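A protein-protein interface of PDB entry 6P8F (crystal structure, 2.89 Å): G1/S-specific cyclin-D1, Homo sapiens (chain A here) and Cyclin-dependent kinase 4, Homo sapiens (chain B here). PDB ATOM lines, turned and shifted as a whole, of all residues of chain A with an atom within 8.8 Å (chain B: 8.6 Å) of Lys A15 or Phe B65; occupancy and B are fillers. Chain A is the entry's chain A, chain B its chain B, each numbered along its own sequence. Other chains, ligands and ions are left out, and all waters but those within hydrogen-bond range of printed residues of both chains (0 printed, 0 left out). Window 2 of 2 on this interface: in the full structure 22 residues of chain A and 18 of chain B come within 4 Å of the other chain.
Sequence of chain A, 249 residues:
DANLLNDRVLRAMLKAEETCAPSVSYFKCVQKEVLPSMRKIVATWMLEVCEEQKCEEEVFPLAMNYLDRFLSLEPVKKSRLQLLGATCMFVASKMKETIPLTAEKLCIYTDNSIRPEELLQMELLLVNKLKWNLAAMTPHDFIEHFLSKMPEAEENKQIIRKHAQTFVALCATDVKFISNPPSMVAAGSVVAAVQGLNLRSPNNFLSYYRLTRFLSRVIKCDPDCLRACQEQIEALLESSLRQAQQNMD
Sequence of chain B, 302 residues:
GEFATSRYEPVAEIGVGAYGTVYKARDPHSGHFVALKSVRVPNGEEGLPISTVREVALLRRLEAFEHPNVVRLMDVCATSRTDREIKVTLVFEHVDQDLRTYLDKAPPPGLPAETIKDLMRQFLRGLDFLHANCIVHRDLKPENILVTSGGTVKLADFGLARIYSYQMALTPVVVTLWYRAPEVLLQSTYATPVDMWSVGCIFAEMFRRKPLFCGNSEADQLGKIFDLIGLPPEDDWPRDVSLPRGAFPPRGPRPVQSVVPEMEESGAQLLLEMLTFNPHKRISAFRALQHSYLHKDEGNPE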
ATOM      1  N   ARG A   8      27.372  -5.692  18.726  1.00  0.00           N
ATOM      2  CA  ARG A   8      26.570  -5.249  19.859  1.00  0.00           C
ATOM      3  C   ARG A   8      25.819  -3.958  19.558  1.00  0.00           C
ATOM      4  O   ARG A   8      24.805  -3.678  20.207  1.00  0.00           O
ATOM      5  CB  ARG A   8      27.469  -5.074  21.082  1.00  0.00           C
ATOM      6  CG  ARG A   8      28.174  -6.352  21.490  1.00  0.00           C
ATOM      7  CD  ARG A   8      29.284  -6.080  22.481  1.00  0.00           C
ATOM      8  NE  ARG A   8      28.905  -5.068  23.461  1.00  0.00           N
ATOM      9  CZ  ARG A   8      29.580  -3.943  23.671  1.00  0.00           C
ATOM     10  NH1 ARG A   8      30.673  -3.682  22.965  1.00  0.00           N
ATOM     11  NH2 ARG A   8      29.166  -3.080  24.588  1.00  0.00           N
ATOM     12  N   VAL A   9      26.290  -3.174  18.587  1.00  0.00           N
ATOM     13  CA  VAL A   9      25.599  -1.943  18.215  1.00  0.00           C
ATOM     14  C   VAL A   9      24.298  -2.263  17.491  1.00  0.00           C
ATOM     15  O   VAL A   9      23.254  -1.655  17.758  1.00  0.00           O
ATOM     16  CB  VAL A   9      26.525  -1.057  17.360  1.00  0.00           C
ATOM     17  CG1 VAL A   9      25.718  -0.050  16.560  1.00  0.00           C
ATOM     18  CG2 VAL A   9      27.554  -0.362  18.242  1.00  0.00           C
ATOM     19  N   LEU A  10      24.341  -3.218  16.558  1.00  0.00           N
ATOM     20  CA  LEU A  10      23.125  -3.671  15.892  1.00  0.00           C
ATOM     21  C   LEU A  10      22.112  -4.203  16.890  1.00  0.00           C
ATOM     22  O   LEU A  10      20.902  -4.043  16.695  1.00  0.00           O
ATOM     23  CB  LEU A  10      23.472  -4.753  14.877  1.00  0.00           C
ATOM     24  CG  LEU A  10      22.663  -4.886  13.595  1.00  0.00           C
ATOM     25  CD1 LEU A  10      22.098  -3.547  13.167  1.00  0.00           C
ATOM     26  CD2 LEU A  10      23.614  -5.422  12.544  1.00  0.00           C
ATOM     27  N   ARG A  11      22.587  -4.845  17.957  1.00  0.00           N
ATOM     28  CA  ARG A  11      21.686  -5.331  18.992  1.00  0.00           C
ATOM     29  C   ARG A  11      20.990  -4.175  19.693  1.00  0.00           C
ATOM     30  O   ARG A  11      19.772  -4.211  19.899  1.00  0.00           O
ATOM     31  CB  ARG A  11      22.464  -6.185  19.992  1.00  0.00           C
ATOM     32  CG  ARG A  11      21.623  -6.810  21.085  1.00  0.00           C
ATOM     33  CD  ARG A  11      22.138  -8.194  21.430  1.00  0.00           C
ATOM     34  NE  ARG A  11      22.279  -8.377  22.867  1.00  0.00           N
ATOM     35  CZ  ARG A  11      21.261  -8.576  23.696  1.00  0.00           C
ATOM     36  NH1 ARG A  11      20.020  -8.615  23.229  1.00  0.00           N
ATOM     37  NH2 ARG A  11      21.482  -8.736  24.995  1.00  0.00           N
ATOM     38  N   ALA A  12      21.750  -3.137  20.056  1.00  0.00           N
ATOM     39  CA  ALA A  12      21.164  -1.984  20.735  1.00  0.00           C
ATOM     40  C   ALA A  12      20.150  -1.279  19.846  1.00  0.00           C
ATOM     41  O   ALA A  12      19.113  -0.808  20.327  1.00  0.00           O
ATOM     42  CB  ALA A  12      22.258  -1.010  21.167  1.00  0.00           C
ATOM     43  N   MET A  13      20.429  -1.205  18.543  1.00  0.00           N
ATOM     44  CA  MET A  13      19.556  -0.466  17.636  1.00  0.00           C
ATOM     45  C   MET A  13      18.191  -1.130  17.523  1.00  0.00           C
ATOM     46  O   MET A  13      17.155  -0.457  17.555  1.00  0.00           O
ATOM     47  CB  MET A  13      20.212  -0.338  16.261  1.00  0.00           C
ATOM     48  CG  MET A  13      21.427   0.568  16.250  1.00  0.00           C
ATOM     49  SD  MET A  13      22.366   0.458  14.722  1.00  0.00           S
ATOM     50  CE  MET A  13      22.184   2.122  14.084  1.00  0.00           C
ATOM     51  N   LEU A  14      18.169  -2.455  17.385  1.00  0.00           N
ATOM     52  CA  LEU A  14      16.892  -3.155  17.321  1.00  0.00           C
ATOM     53  C   LEU A  14      16.121  -3.015  18.625  1.00  0.00           C
ATOM     54  O   LEU A  14      14.886  -2.979  18.615  1.00  0.00           O
ATOM     55  CB  LEU A  14      17.124  -4.626  16.980  1.00  0.00           C
ATOM     56  CG  LEU A  14      17.843  -4.824  15.647  1.00  0.00           C
ATOM     57  CD1 LEU A  14      18.578  -6.163  15.594  1.00  0.00           C
ATOM     58  CD2 LEU A  14      16.846  -4.685  14.503  1.00  0.00           C
ATOM     59  N   LYS A  15      16.828  -2.927  19.753  1.00  0.00           N
ATOM     60  CA  LYS A  15      16.158  -2.698  21.027  1.00  0.00           C
ATOM     61  C   LYS A  15      15.650  -1.265  21.125  1.00  0.00           C
ATOM     62  O   LYS A  15      14.552  -1.019  21.639  1.00  0.00           O
ATOM     63  CB  LYS A  15      17.110  -3.017  22.180  1.00  0.00           C
ATOM     64  CG  LYS A  15      16.536  -2.742  23.560  1.00  0.00           C
ATOM     65  CD  LYS A  15      15.499  -3.782  23.955  1.00  0.00           C
ATOM     66  CE  LYS A  15      14.937  -3.499  25.341  1.00  0.00           C
ATOM     67  NZ  LYS A  15      14.117  -2.256  25.366  1.00  0.00           N
ATOM     68  N   ALA A  16      16.429  -0.306  20.622  1.00  0.00           N
ATOM     69  CA  ALA A  16      16.038   1.093  20.741  1.00  0.00           C
ATOM     70  C   ALA A  16      14.882   1.438  19.813  1.00  0.00           C
ATOM     71  O   ALA A  16      14.117   2.364  20.100  1.00  0.00           O
ATOM     72  CB  ALA A  16      17.239   1.997  20.460  1.00  0.00           C
ATOM     73  N   GLU A  17      14.733   0.711  18.705  1.00  0.00           N
ATOM     74  CA  GLU A  17      13.686   1.014  17.737  1.00  0.00           C
ATOM     75  C   GLU A  17      12.319   0.486  18.154  1.00  0.00           C
ATOM     76  O   GLU A  17      11.351   0.647  17.400  1.00  0.00           O
ATOM     77  CB  GLU A  17      14.065   0.466  16.357  1.00  0.00           C
ATOM     78  CG  GLU A  17      13.912  -1.037  16.200  1.00  0.00           C
ATOM     79  CD  GLU A  17      13.963  -1.491  14.745  1.00  0.00           C
ATOM     80  OE1 GLU A  17      13.916  -0.627  13.845  1.00  0.00           O
ATOM     81  OE2 GLU A  17      14.046  -2.711  14.501  1.00  0.00           O
ATOM     82  N   GLU A  18      12.215  -0.138  19.323  1.00  0.00           N
ATOM     83  CA  GLU A  18      10.934  -0.515  19.899  1.00  0.00           C
ATOM     84  C   GLU A  18      10.365   0.580  20.793  1.00  0.00           C
ATOM     85  O   GLU A  18       9.236   0.446  21.275  1.00  0.00           O
ATOM     86  CB  GLU A  18      11.082  -1.825  20.684  1.00  0.00           C
ATOM     87  CG  GLU A  18      11.839  -2.906  19.916  1.00  0.00           C
ATOM     88  CD  GLU A  18      12.053  -4.185  20.716  1.00  0.00           C
ATOM     89  OE1 GLU A  18      12.272  -4.107  21.946  1.00  0.00           O
ATOM     90  OE2 GLU A  18      12.014  -5.276  20.108  1.00  0.00           O
ATOM     91  N   THR A  19      11.123   1.660  21.007  1.00  0.00           N
ATOM     92  CA  THR A  19      10.694   2.764  21.856  1.00  0.00           C
ATOM     93  C   THR A  19       9.707   3.671  21.133  1.00  0.00           C
ATOM     94  O   THR A  19       8.604   3.926  21.627  1.00  0.00           O
ATOM     95  CB  THR A  19      11.914   3.571  22.306  1.00  0.00           C
ATOM     96  OG1 THR A  19      13.024   2.693  22.507  1.00  0.00           O
ATOM     97  CG2 THR A  19      11.628   4.318  23.591  1.00  0.00           C
ATOM     98  N   CYS A  20      10.091   4.170  19.964  1.00  0.00           N
ATOM     99  CA  CYS A  20       9.318   5.189  19.251  1.00  0.00           C
ATOM    100  C   CYS A  20       8.572   4.572  18.069  1.00  0.00           C
ATOM    101  O   CYS A  20       8.804   4.895  16.903  1.00  0.00           O
ATOM    102  CB  CYS A  20      10.240   6.321  18.794  1.00  0.00           C
ATOM    103  SG  CYS A  20      11.516   6.825  20.001  1.00  0.00           S
ATOM    104  N   ASN A 133      10.733  11.842  23.904  1.00  0.00           N
ATOM    105  CA  ASN A 133      11.379  10.714  23.234  1.00  0.00           C
ATOM    106  C   ASN A 133      11.530  11.051  21.753  1.00  0.00           C
ATOM    107  O   ASN A 133      10.756  10.621  20.898  1.00  0.00           O
ATOM    108  CB  ASN A 133      10.570   9.441  23.440  1.00  0.00           C
ATOM    109  CG  ASN A 133      11.066   8.624  24.599  1.00  0.00           C
ATOM    110  OD1 ASN A 133      10.435   8.573  25.654  1.00  0.00           O
ATOM    111  ND2 ASN A 133      12.211   7.977  24.414  1.00  0.00           N
ATOM    112  N   ALA A 135      14.820  11.027  20.028  1.00  0.00           N
ATOM    113  CA  ALA A 135      15.968  10.409  19.361  1.00  0.00           C
ATOM    114  C   ALA A 135      15.578   9.021  18.846  1.00  0.00           C
ATOM    115  O   ALA A 135      16.082   7.983  19.282  1.00  0.00           O
ATOM    116  CB  ALA A 135      17.163  10.346  20.304  1.00  0.00           C
ATOM    117  N   MET A 137      15.199   5.857  16.322  1.00  0.00           N
ATOM    118  CA  MET A 137      16.051   5.183  15.355  1.00  0.00           C
ATOM    119  C   MET A 137      15.555   5.473  13.943  1.00  0.00           C
ATOM    120  O   MET A 137      14.372   5.306  13.634  1.00  0.00           O
ATOM    121  CB  MET A 137      16.074   3.675  15.618  1.00  0.00           C
ATOM    122  CG  MET A 137      16.738   3.263  16.928  1.00  0.00           C
ATOM    123  SD  MET A 137      18.362   4.014  17.193  1.00  0.00           S
ATOM    124  CE  MET A 137      19.279   3.360  15.808  1.00  0.00           C
ATOM    125  N   PHE A 142      20.076   2.611  10.150  1.00  0.00           N
ATOM    126  CA  PHE A 142      20.258   1.214   9.791  1.00  0.00           C
ATOM    127  C   PHE A 142      20.932   1.064   8.432  1.00  0.00           C
ATOM    128  O   PHE A 142      21.795   0.195   8.264  1.00  0.00           O
ATOM    129  CB  PHE A 142      18.914   0.492   9.824  1.00  0.00           C
ATOM    130  CG  PHE A 142      18.398   0.238  11.213  1.00  0.00           C
ATOM    131  CD1 PHE A 142      17.451   1.071  11.776  1.00  0.00           C
ATOM    132  CD2 PHE A 142      18.857  -0.837  11.956  1.00  0.00           C
ATOM    133  CE1 PHE A 142      16.969   0.839  13.055  1.00  0.00           C
ATOM    134  CE2 PHE A 142      18.379  -1.075  13.233  1.00  0.00           C
ATOM    135  CZ  PHE A 142      17.433  -0.236  13.782  1.00  0.00           C
ATOM    136  N   SER A 183      14.350  -0.644  10.909  1.00  0.00           N
ATOM    137  CA  SER A 183      15.222  -1.712  10.426  1.00  0.00           C
ATOM    138  C   SER A 183      14.653  -2.356   9.169  1.00  0.00           C
ATOM    139  O   SER A 183      15.368  -2.554   8.179  1.00  0.00           O
ATOM    140  CB  SER A 183      15.411  -2.765  11.518  1.00  0.00           C
ATOM    141  OG  SER A 183      14.213  -3.503  11.714  1.00  0.00           O
ATOM    142  N   LYS A 220      16.395 -10.211  12.024  1.00  0.00           N
ATOM    143  CA  LYS A 220      15.587 -11.261  12.652  1.00  0.00           C
ATOM    144  C   LYS A 220      14.217 -11.405  11.982  1.00  0.00           C
ATOM    145  O   LYS A 220      13.167 -11.269  12.613  1.00  0.00           O
ATOM    146  CB  LYS A 220      15.458 -11.010  14.159  1.00  0.00           C
ATOM    147  CG  LYS A 220      16.801 -10.811  14.860  1.00  0.00           C
ATOM    148  CD  LYS A 220      16.640 -10.651  16.369  1.00  0.00           C
ATOM    149  CE  LYS A 220      16.295 -11.968  17.046  1.00  0.00           C
ATOM    150  NZ  LYS A 220      15.610 -11.758  18.355  1.00  0.00           N
ATOM    151  N   LEU B  58      18.457  12.667  24.262  1.00  0.00           N
ATOM    152  CA  LEU B  58      19.512  11.674  24.428  1.00  0.00           C
ATOM    153  C   LEU B  58      19.378  10.952  25.759  1.00  0.00           C
ATOM    154  O   LEU B  58      19.582   9.735  25.836  1.00  0.00           O
ATOM    155  CB  LEU B  58      20.880  12.339  24.315  1.00  0.00           C
ATOM    156  CG  LEU B  58      22.073  11.493  24.767  1.00  0.00           C
ATOM    157  CD1 LEU B  58      22.515  10.530  23.669  1.00  0.00           C
ATOM    158  CD2 LEU B  58      23.222  12.389  25.209  1.00  0.00           C
ATOM    159  N   LEU B  59      19.034  11.686  26.820  1.00  0.00           N
ATOM    160  CA  LEU B  59      18.750  11.034  28.093  1.00  0.00           C
ATOM    161  C   LEU B  59      17.555  10.096  27.970  1.00  0.00           C
ATOM    162  O   LEU B  59      17.568   8.994  28.525  1.00  0.00           O
ATOM    163  CB  LEU B  59      18.512  12.076  29.189  1.00  0.00           C
ATOM    164  CG  LEU B  59      19.745  12.827  29.707  1.00  0.00           C
ATOM    165  CD1 LEU B  59      19.425  13.506  31.030  1.00  0.00           C
ATOM    166  CD2 LEU B  59      20.960  11.909  29.844  1.00  0.00           C
ATOM    167  N   ARG B  60      16.527  10.499  27.223  1.00  0.00           N
ATOM    168  CA  ARG B  60      15.347   9.654  27.082  1.00  0.00           C
ATOM    169  C   ARG B  60      15.665   8.381  26.308  1.00  0.00           C
ATOM    170  O   ARG B  60      15.128   7.311  26.618  1.00  0.00           O
ATOM    171  CB  ARG B  60      14.223  10.438  26.407  1.00  0.00           C
ATOM    172  CG  ARG B  60      13.419  11.288  27.360  1.00  0.00           C
ATOM    173  CD  ARG B  60      12.828  10.426  28.457  1.00  0.00           C
ATOM    174  NE  ARG B  60      11.595  10.993  28.988  1.00  0.00           N
ATOM    175  CZ  ARG B  60      10.730  10.318  29.736  1.00  0.00           C
ATOM    176  NH1 ARG B  60      10.966   9.048  30.035  1.00  0.00           N
ATOM    177  NH2 ARG B  60       9.630  10.911  30.179  1.00  0.00           N
ATOM    178  N   ARG B  61      16.539   8.473  25.303  1.00  0.00           N
ATOM    179  CA  ARG B  61      16.922   7.285  24.543  1.00  0.00           C
ATOM    180  C   ARG B  61      17.584   6.244  25.437  1.00  0.00           C
ATOM    181  O   ARG B  61      17.371   5.039  25.257  1.00  0.00           O
ATOM    182  CB  ARG B  61      17.857   7.669  23.392  1.00  0.00           C
ATOM    183  CG  ARG B  61      18.205   6.508  22.464  1.00  0.00           C
ATOM    184  CD  ARG B  61      18.826   6.985  21.162  1.00  0.00           C
ATOM    185  NE  ARG B  61      20.238   7.316  21.313  1.00  0.00           N
ATOM    186  CZ  ARG B  61      21.228   6.440  21.173  1.00  0.00           C
ATOM    187  NH1 ARG B  61      20.960   5.172  20.881  1.00  0.00           N
ATOM    188  NH2 ARG B  61      22.485   6.830  21.327  1.00  0.00           N
ATOM    189  N   LEU B  62      18.384   6.694  26.411  1.00  0.00           N
ATOM    190  CA  LEU B  62      19.144   5.773  27.252  1.00  0.00           C
ATOM    191  C   LEU B  62      18.229   4.851  28.057  1.00  0.00           C
ATOM    192  O   LEU B  62      18.500   3.647  28.182  1.00  0.00           O
ATOM    193  CB  LEU B  62      20.060   6.557  28.195  1.00  0.00           C
ATOM    194  CG  LEU B  62      21.294   7.301  27.712  1.00  0.00           C
ATOM    195  CD1 LEU B  62      22.103   7.699  28.934  1.00  0.00           C
ATOM    196  CD2 LEU B  62      22.109   6.415  26.796  1.00  0.00           C
ATOM    197  N   GLU B  63      17.145   5.400  28.619  1.00  0.00           N
ATOM    198  CA  GLU B  63      16.295   4.657  29.550  1.00  0.00           C
ATOM    199  C   GLU B  63      15.399   3.645  28.846  1.00  0.00           C
ATOM    200  O   GLU B  63      14.702   2.872  29.526  1.00  0.00           O
ATOM    201  CB  GLU B  63      15.438   5.653  30.363  1.00  0.00           C
ATOM    202  CG  GLU B  63      16.144   6.271  31.604  1.00  0.00           C
ATOM    203  CD  GLU B  63      17.342   7.154  31.285  1.00  0.00           C
ATOM    204  OE1 GLU B  63      17.898   7.057  30.179  1.00  0.00           O
ATOM    205  OE2 GLU B  63      17.739   7.942  32.165  1.00  0.00           O
ATOM    206  N   ALA B  64      15.367   3.665  27.506  1.00  0.00           N
ATOM    207  CA  ALA B  64      14.765   2.559  26.776  1.00  0.00           C
ATOM    208  C   ALA B  64      15.436   1.236  27.123  1.00  0.00           C
ATOM    209  O   ALA B  64      14.797   0.176  27.067  1.00  0.00           O
ATOM    210  CB  ALA B  64      14.853   2.823  25.280  1.00  0.00           C
ATOM    211  N   PHE B  65      16.726   1.271  27.459  1.00  0.00           N
ATOM    212  CA  PHE B  65      17.452   0.073  27.855  1.00  0.00           C
ATOM    213  C   PHE B  65      17.370  -0.198  29.349  1.00  0.00           C
ATOM    214  O   PHE B  65      17.588  -1.343  29.769  1.00  0.00           O
ATOM    215  CB  PHE B  65      18.918   0.191  27.434  1.00  0.00           C
ATOM    216  CG  PHE B  65      19.100   0.509  25.980  1.00  0.00           C
ATOM    217  CD1 PHE B  65      19.006  -0.488  25.024  1.00  0.00           C
ATOM    218  CD2 PHE B  65      19.354   1.805  25.569  1.00  0.00           C
ATOM    219  CE1 PHE B  65      19.170  -0.198  23.678  1.00  0.00           C
ATOM    220  CE2 PHE B  65      19.516   2.103  24.232  1.00  0.00           C
ATOM    221  CZ  PHE B  65      19.424   1.098  23.283  1.00  0.00           C
ATOM    222  N   GLU B  66      17.049   0.819  30.152  1.00  0.00           N
ATOM    223  CA  GLU B  66      17.009   0.715  31.612  1.00  0.00           C
ATOM    224  C   GLU B  66      18.270   0.024  32.141  1.00  0.00           C
ATOM    225  O   GLU B  66      18.243  -1.112  32.614  1.00  0.00           O
ATOM    226  CB  GLU B  66      15.748  -0.027  32.075  1.00  0.00           C
ATOM    227  CG  GLU B  66      14.466   0.463  31.436  1.00  0.00           C
ATOM    228  CD  GLU B  66      13.365   0.714  32.448  1.00  0.00           C
ATOM    229  OE1 GLU B  66      12.659   1.735  32.310  1.00  0.00           O
ATOM    230  OE2 GLU B  66      13.193  -0.114  33.369  1.00  0.00           O
ATOM    231  N   HIS B  67      19.388   0.734  32.029  1.00  0.00           N
ATOM    232  CA  HIS B  67      20.643   0.118  32.441  1.00  0.00           C
ATOM    233  C   HIS B  67      20.804   0.231  33.952  1.00  0.00           C
ATOM    234  O   HIS B  67      20.612   1.314  34.512  1.00  0.00           O
ATOM    235  CB  HIS B  67      21.841   0.749  31.742  1.00  0.00           C
ATOM    236  CG  HIS B  67      23.072  -0.105  31.799  1.00  0.00           C
ATOM    237  ND1 HIS B  67      23.830  -0.243  32.943  1.00  0.00           N
ATOM    238  CD2 HIS B  67      23.657  -0.891  30.863  1.00  0.00           C
ATOM    239  CE1 HIS B  67      24.835  -1.066  32.705  1.00  0.00           C
ATOM    240  NE2 HIS B  67      24.754  -1.473  31.450  1.00  0.00           N
ATOM    241  N   PRO B  68      21.169  -0.857  34.636  1.00  0.00           N
ATOM    242  CA  PRO B  68      21.208  -0.828  36.106  1.00  0.00           C
ATOM    243  C   PRO B  68      22.379  -0.056  36.701  1.00  0.00           C
ATOM    244  O   PRO B  68      22.345   0.214  37.906  1.00  0.00           O
ATOM    245  CB  PRO B  68      21.281  -2.314  36.477  1.00  0.00           C
ATOM    246  CG  PRO B  68      21.920  -2.958  35.301  1.00  0.00           C
ATOM    247  CD  PRO B  68      21.427  -2.206  34.103  1.00  0.00           C
ATOM    248  N   ARG B  72      18.480   6.284  36.335  1.00  0.00           N
ATOM    249  CA  ARG B  72      17.403   6.339  35.362  1.00  0.00           C
ATOM    250  C   ARG B  72      16.649   7.658  35.479  1.00  0.00           C
ATOM    251  O   ARG B  72      16.410   8.157  36.583  1.00  0.00           O
ATOM    252  CB  ARG B  72      16.446   5.162  35.558  1.00  0.00           C
ATOM    253  CG  ARG B  72      16.765   3.957  34.688  1.00  0.00           C
ATOM    254  CD  ARG B  72      15.987   2.714  35.117  1.00  0.00           C
ATOM    255  NE  ARG B  72      14.679   3.017  35.697  1.00  0.00           N
ATOM    256  CZ  ARG B  72      13.619   3.415  34.996  1.00  0.00           C
ATOM    257  NH1 ARG B  72      13.708   3.577  33.682  1.00  0.00           N
ATOM    258  NH2 ARG B  72      12.469   3.660  35.609  1.00  0.00           N
ATOM    259  N   PHE B 129      28.094   1.233  28.699  1.00  0.00           N
ATOM    260  CA  PHE B 129      26.764   1.551  28.193  1.00  0.00           C
ATOM    261  C   PHE B 129      26.717   2.975  27.654  1.00  0.00           C
ATOM    262  O   PHE B 129      26.182   3.224  26.568  1.00  0.00           O
ATOM    263  CB  PHE B 129      25.721   1.350  29.293  1.00  0.00           C
ATOM    264  CG  PHE B 129      24.347   1.831  28.919  1.00  0.00           C
ATOM    265  CD1 PHE B 129      23.552   1.098  28.053  1.00  0.00           C
ATOM    266  CD2 PHE B 129      23.851   3.023  29.429  1.00  0.00           C
ATOM    267  CE1 PHE B 129      22.285   1.543  27.702  1.00  0.00           C
ATOM    268  CE2 PHE B 129      22.586   3.473  29.081  1.00  0.00           C
ATOM    269  CZ  PHE B 129      21.804   2.733  28.218  1.00  0.00           C
ATOM    270  N   ALA B 132      28.752   3.347  24.429  1.00  0.00           N
ATOM    271  CA  ALA B 132      28.035   2.716  23.327  1.00  0.00           C
ATOM    272  C   ALA B 132      26.893   3.580  22.814  1.00  0.00           C
ATOM    273  O   ALA B 132      26.422   3.368  21.691  1.00  0.00           O
ATOM    274  CB  ALA B 132      27.510   1.349  23.758  1.00  0.00           C
ATOM    275  N   ASN B 133      26.436   4.548  23.604  1.00  0.00           N
ATOM    276  CA  ASN B 133      25.433   5.504  23.163  1.00  0.00           C
ATOM    277  C   ASN B 133      26.033   6.896  22.983  1.00  0.00           C
ATOM    278  O   ASN B 133      25.345   7.907  23.152  1.00  0.00           O
ATOM    279  CB  ASN B 133      24.251   5.523  24.130  1.00  0.00           C
ATOM    280  CG  ASN B 133      23.394   4.269  24.017  1.00  0.00           C
ATOM    281  OD1 ASN B 133      22.652   4.093  23.048  1.00  0.00           O
ATOM    282  ND2 ASN B 133      23.510   3.385  24.998  1.00  0.00           N
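Printed residues of chain B within 4 Å of Ala A12: Phe B65 (3.4 Å). Ala A16 touches just one residue of chain B: Phe B65. Of the printed residues of chain B, Asn A133 touches Arg B60. Printed residues of chain B within 4 Å of Ala A135: Arg B61. Of the printed residues of chain A, Arg B61 touches Ala A135 (3.5 Å). Leu B62 touches none of the printed residues of chain A. Of chain A, only Lys A15 and Thr A19 come within 4 Å of Ala B64. His B67 touches none of the printed residues of chain A. The nearest printed residue of chain B that does not touch Asn A133 is Arg B61 (4.4 Å).
O of Ala B64 lies within hydrogen-bond range of NZ of Lys A15 (3.0 Å).
Of the 19 printed residues of chain A, 6 touch a printed residue of chain B. Of the 15 printed residues of chain B, 4 touch a printed residue of chain A. Hydrophobic or aromatic side chains of chain B that line the printed part of chain A: Ala B64 and Phe B65. Among the printed residues, no Asp or Glu carboxylate lies within 4 Å of a Lys or Arg side-chain nitrogen of the other chain.
O of Ala A16 is in hydrogen-bond range of OG1 of Thr A19, at 2.7 Å. The guanidinium group of Arg B61 is in hydrogen-bond range of the side-chain amide oxygen of Asn B133 (3.0 Å).
Among the printed residues, pairs that only touch across the chains: Thr A19 with Ala B64, Ala A12 with Phe B65, Ala A135 with Arg B61, Lys A15 with Phe B65, Ala A16 with Phe B65 and Asn A133 with Arg B60.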
